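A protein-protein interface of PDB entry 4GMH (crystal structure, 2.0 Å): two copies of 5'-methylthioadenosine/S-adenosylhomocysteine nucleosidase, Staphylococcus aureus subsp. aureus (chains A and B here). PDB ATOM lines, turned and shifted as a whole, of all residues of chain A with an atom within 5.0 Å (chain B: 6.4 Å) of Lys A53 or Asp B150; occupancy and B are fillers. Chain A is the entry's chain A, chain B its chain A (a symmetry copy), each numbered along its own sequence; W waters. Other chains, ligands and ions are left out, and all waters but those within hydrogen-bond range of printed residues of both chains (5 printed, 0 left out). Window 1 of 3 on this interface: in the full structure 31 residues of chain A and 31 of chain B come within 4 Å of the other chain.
The side-chain amino group (NZ) of Lys A53 lies within salt-bridge range of the side-chain carboxylate (OD2) of Asp B150 (2.9 Å). N of Asp A102 sits at hydrogen-bond distance from O of Asp B150 (3.2 Å). The backbone NH of Asp A102 sits at hydrogen-bond distance from the side-chain hydroxyl of Ser B151 (3.5 Å). N of Phe B152 sits at hydrogen-bond distance from O of Asp A102. The side-chain amino group of Lys B53 lies within salt-bridge range of the side-chain carboxylate of Asp A150.
O of Ile A51 is in hydrogen-bond range of ND2 of Asn A55, 3.2 Å away. The side-chain amino group (NZ) of Lys A53 is in salt-bridge range of the side-chain carboxylate (OD1) of Asp A100 (3.0 Å). The backbone NH (N) of Lys A53 sits at hydrogen-bond distance from the side-chain carboxylate (OD1) of Asp A150, 3.0 Å away. The backbone NH (N) of Asp A150 lies within hydrogen-bond range of the side-chain carboxylate (OD2) of Asp A100 (3.0 Å). The side-chain amino group (NZ) of Lys B53 is in salt-bridge range of the side-chain carboxylate (OD1) of Asp B100, 3.0 Å away. The backbone NH (N) of Asp B150 lies within hydrogen-bond range of the side-chain carboxylate (OD2) of Asp B100.
Among the printed residues, merely in contact across the chains: Ala A101 with Asp B150 (3.2 Å), Tyr A98 with Val B54 (3.4 Å), Ile A51 with Ile B113 (3.5 Å), Ile A113 with Ile B51 (3.5 Å), Ala A178 with Val B54 (3.7 Å), Asp A100 with Ser B151 (3.8 Å), Ala A57 with Val B54 (3.98 Å) and Val A54 with Ala B57 (3.98 Å).
Of the printed residues of chain B, Lys A53 touches Asp B150. Of the printed residues of chain A, Asp B150 touches Lys A53, Ala A101 and Asp A102. Of the printed residues of chain B, Ile A51 touches Ile B113. Of the printed residues of chain B, Tyr A98 touches Val B54 (3.4 Å). Of the printed residues of chain A, Phe B152 touches Asp A102 (3.1 Å).
Printed residues of chain B that touch a printed residue of chain A: Ile B51, Lys B53, Val B54, Ala B57, Ile B113, Asp B150, Ser B151 and Phe B152. Hydrophobic or aromatic side chains of chain B within 4 Å of the printed part of chain A: Val B54, Ala B57 and Ile B113. Printed residues of chain A that touch a printed residue of chain B: Ile A51, Lys A53, Val A54, Ala A57, Tyr A98, Asp A100, Ala A101, Asp A102, Ile A113, Asp A150 and Ala A178. Hydrophobic or aromatic side chains of chain A within 4 Å of the printed part of chain B: Val A54, Ala A57, Tyr A98, Ala A101, Ile A113 and Ala A178. Among the printed residues, 13 pairs touch across the chains. Among the printed residues, Asp or Glu carboxylates within 4 Å of a Lys or Arg side-chain nitrogen of the other chain: Lys A53 with Asp B150 and Asp A150 with Lys B53.
Ile A51 touches Ile B113, and with the chains exchanged Ile A113 touches Ile B51. Lys A53 touches Asp B150, and with the chains exchanged Asp A150 touches Lys B53. Val A54 touches Ala B57, and with the chains exchanged Ala A57 touches Val B54. Of the 13 pairs that touch across the chains among the printed residues, 6 have their exchanged pair printed and touching as well.
Water W3 lies within hydrogen-bond range of O of Asp B100 and OD2 of Asp A100. Water W5 lies within hydrogen-bond range of the backbone carbonyl oxygen of Asp A100 (2.8 Å), the side-chain hydroxyl of Ser B151 (2.9 Å) and the side-chain carboxylate of Asp B100 (2.9 Å). Water W2 lies within hydrogen-bond range of OD2 of Asp A100 (2.8 Å), OD2 of Asp B100 (2.8 Å), NZ of Lys A53 (3.2 Å) and NZ of Lys B53 (3.2 Å). Water W4 lies within hydrogen-bond range of the backbone carbonyl oxygen of Asp B150 and the backbone NH of Asp A102. Water W1 bridges the backbone carbonyl oxygen (O) of Asp A102 (3.2 Å) and the backbone carbonyl oxygen (O) of Phe B152 (3.4 Å).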
ATOM      1  N   ILE A  51      -1.769   1.630   7.769  1.00  0.00           N
ATOM      2  CA  ILE A  51      -2.658   0.566   8.350  1.00  0.00           C
ATOM      3  C   ILE A  51      -2.239  -0.915   8.049  1.00  0.00           C
ATOM      4  O   ILE A  51      -1.767  -1.212   6.893  1.00  0.00           O
ATOM      5  CB  ILE A  51      -4.138   0.827   7.945  1.00  0.00           C
ATOM      6  CG1 ILE A  51      -4.655   2.135   8.620  1.00  0.00           C
ATOM      7  CG2 ILE A  51      -5.126  -0.341   8.274  1.00  0.00           C
ATOM      8  CD1 ILE A  51      -5.953   2.646   7.974  1.00  0.00           C
ATOM      9  N   GLY A  52      -2.414  -1.838   9.052  1.00  0.00           N
ATOM     10  CA  GLY A  52      -2.112  -3.308   8.824  1.00  0.00           C
ATOM     11  C   GLY A  52      -0.691  -3.783   9.073  1.00  0.00           C
ATOM     12  O   GLY A  52       0.190  -2.949   9.355  1.00  0.00           O
ATOM     13  N   LYS A  53      -0.474  -5.117   9.014  1.00  0.00           N
ATOM     14  CA  LYS A  53       0.713  -5.777   9.608  1.00  0.00           C
ATOM     15  C   LYS A  53       2.044  -5.447   8.910  1.00  0.00           C
ATOM     16  O   LYS A  53       3.032  -5.202   9.601  1.00  0.00           O
ATOM     17  CB  LYS A  53       0.571  -7.359   9.537  1.00  0.00           C
ATOM     18  CG  LYS A  53      -0.462  -8.058  10.416  1.00  0.00           C
ATOM     19  CD  LYS A  53      -0.380  -9.597   9.970  1.00  0.00           C
ATOM     20  CE  LYS A  53      -1.593 -10.322  10.449  1.00  0.00           C
ATOM     21  NZ  LYS A  53      -1.338 -11.801  10.492  1.00  0.00           N
ATOM     22  N   VAL A  54       2.029  -5.419   7.535  1.00  0.00           N
ATOM     23  CA  VAL A  54       3.262  -5.164   6.704  1.00  0.00           C
ATOM     24  C   VAL A  54       3.707  -3.693   6.867  1.00  0.00           C
ATOM     25  O   VAL A  54       4.899  -3.408   7.048  1.00  0.00           O
ATOM     26  CB  VAL A  54       3.101  -5.696   5.207  1.00  0.00           C
ATOM     27  CG1 VAL A  54       4.296  -5.291   4.287  1.00  0.00           C
ATOM     28  CG2 VAL A  54       2.936  -7.254   5.188  1.00  0.00           C
ATOM     29  N   ASN A  55       2.761  -2.720   6.774  1.00  0.00           N
ATOM     30  CA  ASN A  55       3.104  -1.266   6.964  1.00  0.00           C
ATOM     31  C   ASN A  55       3.703  -0.999   8.368  1.00  0.00           C
ATOM     32  O   ASN A  55       4.710  -0.217   8.481  1.00  0.00           O
ATOM     33  CB  ASN A  55       1.880  -0.378   6.767  1.00  0.00           C
ATOM     34  CG  ASN A  55       1.618  -0.013   5.266  1.00  0.00           C
ATOM     35  OD1 ASN A  55       2.553  -0.070   4.437  1.00  0.00           O
ATOM     36  ND2 ASN A  55       0.311   0.197   4.883  1.00  0.00           N
ATOM     37  N   ALA A  56       3.130  -1.640   9.427  1.00  0.00           N
ATOM     38  CA  ALA A  56       3.641  -1.491  10.818  1.00  0.00           C
ATOM     39  C   ALA A  56       5.067  -2.148  10.973  1.00  0.00           C
ATOM     40  O   ALA A  56       6.015  -1.553  11.598  1.00  0.00           O
ATOM     41  CB  ALA A  56       2.585  -2.135  11.805  1.00  0.00           C
ATOM     42  N   ALA A  57       5.267  -3.318  10.330  1.00  0.00           N
ATOM     43  CA  ALA A  57       6.649  -3.954  10.409  1.00  0.00           C
ATOM     44  C   ALA A  57       7.795  -3.177   9.665  1.00  0.00           C
ATOM     45  O   ALA A  57       8.944  -3.072  10.207  1.00  0.00           O
ATOM     46  CB  ALA A  57       6.582  -5.404   9.949  1.00  0.00           C
ATOM     47  N   TYR A  98      -1.876 -13.228  17.305  1.00  0.00           N
ATOM     48  CA  TYR A  98      -2.731 -13.157  16.072  1.00  0.00           C
ATOM     49  C   TYR A  98      -4.054 -13.933  16.213  1.00  0.00           C
ATOM     50  O   TYR A  98      -4.020 -15.069  16.741  1.00  0.00           O
ATOM     51  CB  TYR A  98      -1.960 -13.660  14.797  1.00  0.00           C
ATOM     52  CG  TYR A  98      -0.645 -12.839  14.492  1.00  0.00           C
ATOM     53  CD1 TYR A  98      -0.714 -11.475  14.125  1.00  0.00           C
ATOM     54  CD2 TYR A  98       0.621 -13.460  14.443  1.00  0.00           C
ATOM     55  CE1 TYR A  98       0.428 -10.717  13.793  1.00  0.00           C
ATOM     56  CE2 TYR A  98       1.782 -12.689  14.088  1.00  0.00           C
ATOM     57  CZ  TYR A  98       1.674 -11.322  13.779  1.00  0.00           C
ATOM     58  OH  TYR A  98       2.850 -10.516  13.505  1.00  0.00           O
ATOM     59  N   ASP A 100      -5.735 -14.441  13.260  1.00  0.00           N
ATOM     60  CA  ASP A 100      -5.905 -14.948  11.851  1.00  0.00           C
ATOM     61  C   ASP A 100      -4.726 -15.812  11.253  1.00  0.00           C
ATOM     62  O   ASP A 100      -4.597 -15.886  10.017  1.00  0.00           O
ATOM     63  CB  ASP A 100      -6.277 -13.786  10.873  1.00  0.00           C
ATOM     64  CG  ASP A 100      -5.064 -12.734  10.685  1.00  0.00           C
ATOM     65  OD1 ASP A 100      -3.981 -12.853  11.348  1.00  0.00           O
ATOM     66  OD2 ASP A 100      -5.196 -11.764   9.866  1.00  0.00           O
ATOM     67  N   ALA A 101      -3.838 -16.365  12.100  1.00  0.00           N
ATOM     68  CA  ALA A 101      -2.739 -17.269  11.681  1.00  0.00           C
ATOM     69  C   ALA A 101      -3.184 -18.760  11.924  1.00  0.00           C
ATOM     70  O   ALA A 101      -3.581 -19.096  13.098  1.00  0.00           O
ATOM     71  CB  ALA A 101      -1.438 -16.941  12.434  1.00  0.00           C
ATOM     72  N   ASP A 102      -3.211 -19.598  10.844  1.00  0.00           N
ATOM     73  CA  ASP A 102      -3.529 -21.094  10.941  1.00  0.00           C
ATOM     74  C   ASP A 102      -2.496 -22.076  10.247  1.00  0.00           C
ATOM     75  O   ASP A 102      -2.620 -22.324   9.077  1.00  0.00           O
ATOM     76  CB  ASP A 102      -4.960 -21.350  10.447  1.00  0.00           C
ATOM     77  CG  ASP A 102      -5.438 -22.863  10.673  1.00  0.00           C
ATOM     78  OD1 ASP A 102      -4.688 -23.637  11.270  1.00  0.00           O
ATOM     79  OD2 ASP A 102      -6.555 -23.206  10.235  1.00  0.00           O
ATOM     80  N   ILE A 113       2.719 -18.502  14.588  1.00  0.00           N
ATOM     81  CA  ILE A 113       3.562 -18.477  13.335  1.00  0.00           C
ATOM     82  C   ILE A 113       4.633 -19.587  13.512  1.00  0.00           C
ATOM     83  O   ILE A 113       5.296 -19.620  14.556  1.00  0.00           O
ATOM     84  CB  ILE A 113       4.259 -17.076  13.126  1.00  0.00           C
ATOM     85  CG1 ILE A 113       3.203 -15.972  12.740  1.00  0.00           C
ATOM     86  CG2 ILE A 113       5.356 -17.092  12.003  1.00  0.00           C
ATOM     87  CD1 ILE A 113       2.447 -16.237  11.436  1.00  0.00           C
ATOM     88  N   GLY A 149      -5.214  -8.675  13.549  1.00  0.00           N
ATOM     89  CA  GLY A 149      -5.408  -9.320  12.198  1.00  0.00           C
ATOM     90  C   GLY A 149      -5.497  -8.313  11.030  1.00  0.00           C
ATOM     91  O   GLY A 149      -5.673  -7.105  11.309  1.00  0.00           O
ATOM     92  N   ASP A 150      -5.386  -8.743   9.746  1.00  0.00           N
ATOM     93  CA  ASP A 150      -5.614  -7.773   8.577  1.00  0.00           C
ATOM     94  C   ASP A 150      -7.125  -7.575   8.105  1.00  0.00           C
ATOM     95  O   ASP A 150      -7.377  -7.293   6.909  1.00  0.00           O
ATOM     96  CB  ASP A 150      -4.716  -8.116   7.330  1.00  0.00           C
ATOM     97  CG  ASP A 150      -3.246  -7.487   7.420  1.00  0.00           C
ATOM     98  OD1 ASP A 150      -3.002  -6.610   8.293  1.00  0.00           O
ATOM     99  OD2 ASP A 150      -2.358  -7.934   6.639  1.00  0.00           O
ATOM    100  N   MET A 174      -5.417  -3.887  14.351  1.00  0.00           N
ATOM    101  CA  MET A 174      -4.735  -4.277  13.073  1.00  0.00           C
ATOM    102  C   MET A 174      -3.154  -4.162  13.047  1.00  0.00           C
ATOM    103  O   MET A 174      -2.542  -4.536  11.995  1.00  0.00           O
ATOM    104  CB  MET A 174      -5.406  -3.498  11.857  1.00  0.00           C
ATOM    105  CG  MET A 174      -6.951  -3.737  11.692  1.00  0.00           C
ATOM    106  SD  MET A 174      -7.784  -2.796  10.279  1.00  0.00           S
ATOM    107  CE  MET A 174      -7.159  -3.713   8.883  1.00  0.00           C
ATOM    108  N   ALA A 178       2.118  -7.242  15.215  1.00  0.00           N
ATOM    109  CA  ALA A 178       3.249  -7.033  14.231  1.00  0.00           C
ATOM    110  C   ALA A 178       4.431  -6.163  14.803  1.00  0.00           C
ATOM    111  O   ALA A 178       5.679  -6.441  14.563  1.00  0.00           O
ATOM    112  CB  ALA A 178       2.678  -6.468  12.894  1.00  0.00           C
ATOM    113  N   ILE B  51       9.167 -17.782   8.074  1.00  0.00           N
ATOM    114  CA  ILE B  51       7.802 -17.987   7.479  1.00  0.00           C
ATOM    115  C   ILE B  51       6.750 -16.864   7.776  1.00  0.00           C
ATOM    116  O   ILE B  51       6.729 -16.312   8.935  1.00  0.00           O
ATOM    117  CB  ILE B  51       7.255 -19.391   7.871  1.00  0.00           C
ATOM    118  CG1 ILE B  51       8.113 -20.507   7.199  1.00  0.00           C
ATOM    119  CG2 ILE B  51       5.748 -19.630   7.527  1.00  0.00           C
ATOM    120  CD1 ILE B  51       7.871 -21.886   7.835  1.00  0.00           C
ATOM    121  N   GLY B  52       5.879 -16.531   6.766  1.00  0.00           N
ATOM    122  CA  GLY B  52       4.776 -15.512   6.989  1.00  0.00           C
ATOM    123  C   GLY B  52       5.108 -14.049   6.751  1.00  0.00           C
ATOM    124  O   GLY B  52       6.280 -13.725   6.483  1.00  0.00           O
ATOM    125  N   LYS B  53       4.078 -13.172   6.806  1.00  0.00           N
ATOM    126  CA  LYS B  53       4.135 -11.812   6.219  1.00  0.00           C
ATOM    127  C   LYS B  53       5.100 -10.848   6.931  1.00  0.00           C
ATOM    128  O   LYS B  53       5.827 -10.126   6.251  1.00  0.00           O
ATOM    129  CB  LYS B  53       2.707 -11.114   6.280  1.00  0.00           C
ATOM    130  CG  LYS B  53       1.583 -11.631   5.389  1.00  0.00           C
ATOM    131  CD  LYS B  53       0.305 -10.767   5.826  1.00  0.00           C
ATOM    132  CE  LYS B  53      -0.940 -11.425   5.332  1.00  0.00           C
ATOM    133  NZ  LYS B  53      -2.072 -10.441   5.284  1.00  0.00           N
ATOM    134  N   VAL B  54       5.103 -10.883   8.306  1.00  0.00           N
ATOM    135  CA  VAL B  54       5.951  -9.965   9.150  1.00  0.00           C
ATOM    136  C   VAL B  54       7.442 -10.346   8.999  1.00  0.00           C
ATOM    137  O   VAL B  54       8.305  -9.472   8.831  1.00  0.00           O
ATOM    138  CB  VAL B  54       5.400  -9.835  10.643  1.00  0.00           C
ATOM    139  CG1 VAL B  54       6.356  -9.027  11.576  1.00  0.00           C
ATOM    140  CG2 VAL B  54       3.981  -9.169  10.652  1.00  0.00           C
ATOM    141  N   ALA B  57       8.604  -9.187   5.553  1.00  0.00           N
ATOM    142  CA  ALA B  57       8.776  -7.674   5.484  1.00  0.00           C
ATOM    143  C   ALA B  57      10.027  -7.101   6.243  1.00  0.00           C
ATOM    144  O   ALA B  57      10.717  -6.170   5.712  1.00  0.00           O
ATOM    145  CB  ALA B  57       7.497  -6.983   5.936  1.00  0.00           C
ATOM    146  N   HIS B  99      -5.343 -12.925  -0.067  1.00  0.00           N
ATOM    147  CA  HIS B  99      -6.698 -13.576   0.072  1.00  0.00           C
ATOM    148  C   HIS B  99      -7.354 -13.341   1.480  1.00  0.00           C
ATOM    149  O   HIS B  99      -8.559 -13.677   1.687  1.00  0.00           O
ATOM    150  CB  HIS B  99      -6.676 -15.106  -0.302  1.00  0.00           C
ATOM    151  CG  HIS B  99      -5.854 -15.991   0.645  1.00  0.00           C
ATOM    152  ND1 HIS B  99      -6.337 -16.406   1.873  1.00  0.00           N
ATOM    153  CD2 HIS B  99      -4.628 -16.587   0.504  1.00  0.00           C
ATOM    154  CE1 HIS B  99      -5.434 -17.200   2.467  1.00  0.00           C
ATOM    155  NE2 HIS B  99      -4.388 -17.346   1.642  1.00  0.00           N
ATOM    156  N   ASP B 100      -6.581 -12.820   2.461  1.00  0.00           N
ATOM    157  CA  ASP B 100      -7.117 -12.710   3.865  1.00  0.00           C
ATOM    158  C   ASP B 100      -7.250 -11.257   4.470  1.00  0.00           C
ATOM    159  O   ASP B 100      -7.258 -11.116   5.706  1.00  0.00           O
ATOM    160  CB  ASP B 100      -6.325 -13.635   4.846  1.00  0.00           C
ATOM    161  CG  ASP B 100      -4.798 -13.144   5.051  1.00  0.00           C
ATOM    162  OD1 ASP B 100      -4.333 -12.152   4.398  1.00  0.00           O
ATOM    163  OD2 ASP B 100      -4.044 -13.764   5.873  1.00  0.00           O
ATOM    164  N   ILE B 113      -5.664  -3.479   1.191  1.00  0.00           N
ATOM    165  CA  ILE B 113      -5.217  -2.777   2.452  1.00  0.00           C
ATOM    166  C   ILE B 113      -5.611  -1.285   2.279  1.00  0.00           C
ATOM    167  O   ILE B 113      -5.286  -0.695   1.241  1.00  0.00           O
ATOM    168  CB  ILE B 113      -3.660  -2.908   2.675  1.00  0.00           C
ATOM    169  CG1 ILE B 113      -3.266  -4.385   3.056  1.00  0.00           C
ATOM    170  CG2 ILE B 113      -3.116  -1.966   3.808  1.00  0.00           C
ATOM    171  CD1 ILE B 113      -3.897  -4.901   4.352  1.00  0.00           C
ATOM    172  N   SER B 148      -1.583 -14.575  -1.412  1.00  0.00           N
ATOM    173  CA  SER B 148      -0.847 -14.887  -0.141  1.00  0.00           C
ATOM    174  C   SER B 148      -1.736 -14.691   1.107  1.00  0.00           C
ATOM    175  O   SER B 148      -2.620 -13.829   1.089  1.00  0.00           O
ATOM    176  CB  SER B 148       0.372 -13.898   0.052  1.00  0.00           C
ATOM    177  OG  SER B 148       1.312 -13.918  -1.057  1.00  0.00           O
ATOM    178  N   GLY B 149      -1.376 -15.360   2.207  1.00  0.00           N
ATOM    179  CA  GLY B 149      -2.042 -15.198   3.553  1.00  0.00           C
ATOM    180  C   GLY B 149      -1.238 -15.803   4.726  1.00  0.00           C
ATOM    181  O   GLY B 149      -0.293 -16.578   4.452  1.00  0.00           O
ATOM    182  N   ASP B 150      -1.560 -15.492   6.008  1.00  0.00           N
ATOM    183  CA  ASP B 150      -0.859 -16.196   7.180  1.00  0.00           C
ATOM    184  C   ASP B 150      -1.477 -17.593   7.639  1.00  0.00           C
ATOM    185  O   ASP B 150      -1.378 -17.961   8.834  1.00  0.00           O
ATOM    186  CB  ASP B 150      -0.700 -15.256   8.433  1.00  0.00           C
ATOM    187  CG  ASP B 150       0.601 -14.324   8.361  1.00  0.00           C
ATOM    188  OD1 ASP B 150       1.486 -14.565   7.495  1.00  0.00           O
ATOM    189  OD2 ASP B 150       0.671 -13.337   9.147  1.00  0.00           O
ATOM    190  N   SER B 151      -2.062 -18.351   6.700  1.00  0.00           N
ATOM    191  CA  SER B 151      -2.513 -19.772   6.886  1.00  0.00           C
ATOM    192  C   SER B 151      -1.945 -20.784   5.781  1.00  0.00           C
ATOM    193  O   SER B 151      -1.650 -20.381   4.590  1.00  0.00           O
ATOM    194  CB  SER B 151      -4.063 -19.836   6.850  1.00  0.00           C
ATOM    195  OG  SER B 151      -4.696 -18.956   7.793  1.00  0.00           O
ATOM    196  N   PHE B 152      -1.743 -22.041   6.169  1.00  0.00           N
ATOM    197  CA  PHE B 152      -1.495 -23.176   5.262  1.00  0.00           C
ATOM    198  C   PHE B 152      -2.852 -23.754   4.812  1.00  0.00           C
ATOM    199  O   PHE B 152      -3.729 -24.085   5.656  1.00  0.00           O
ATOM    200  CB  PHE B 152      -0.629 -24.277   5.949  1.00  0.00           C
ATOM    201  CG  PHE B 152      -0.171 -25.404   4.988  1.00  0.00           C
ATOM    202  CD1 PHE B 152       0.885 -25.206   4.087  1.00  0.00           C
ATOM    203  CD2 PHE B 152      -0.817 -26.648   4.979  1.00  0.00           C
ATOM    204  CE1 PHE B 152       1.282 -26.225   3.205  1.00  0.00           C
ATOM    205  CE2 PHE B 152      -0.447 -27.673   4.089  1.00  0.00           C
ATOM    206  CZ  PHE B 152       0.611 -27.465   3.195  1.00  0.00           C
ATOM    207  N   GLU B 173       0.278 -19.259  -1.295  1.00  0.00           N
ATOM    208  CA  GLU B 173       1.498 -19.412  -0.368  1.00  0.00           C
ATOM    209  C   GLU B 173       1.473 -18.276   0.743  1.00  0.00           C
ATOM    210  O   GLU B 173       0.353 -17.664   0.984  1.00  0.00           O
ATOM    211  CB  GLU B 173       2.873 -19.554  -1.193  1.00  0.00           C
ATOM    212  CG  GLU B 173       3.077 -18.477  -2.329  1.00  0.00           C
ATOM    213  CD  GLU B 173       3.176 -17.080  -1.713  1.00  0.00           C
ATOM    214  OE1 GLU B 173       4.251 -16.694  -1.114  1.00  0.00           O
ATOM    215  OE2 GLU B 173       2.189 -16.328  -1.790  1.00  0.00           O
ATOM    216  N   MET B 174       2.621 -18.009   1.428  1.00  0.00           N
ATOM    217  CA  MET B 174       2.628 -17.231   2.711  1.00  0.00           C
ATOM    218  C   MET B 174       3.545 -15.938   2.753  1.00  0.00           C
ATOM    219  O   MET B 174       3.533 -15.226   3.809  1.00  0.00           O
ATOM    220  CB  MET B 174       2.936 -18.215   3.925  1.00  0.00           C
ATOM    221  CG  MET B 174       1.929 -19.413   4.074  1.00  0.00           C
ATOM    222  SD  MET B 174       2.290 -20.621   5.484  1.00  0.00           S
ATOM    223  CE  MET B 174       1.816 -19.618   6.881  1.00  0.00           C
HETATM  224  O   HOH W   1      -3.247 -25.454   8.783  1.00  0.00           O
HETATM  225  O   HOH W   2      -3.170 -11.946   7.879  1.00  0.00           O
HETATM  226  O   HOH W   3      -7.746 -11.325   8.496  1.00  0.00           O
HETATM  227  O   HOH W   4       0.180 -19.637  10.654  1.00  0.00           O
HETATM  228  O   HOH W   5      -5.003 -16.180   7.223  1.00  0.00           O
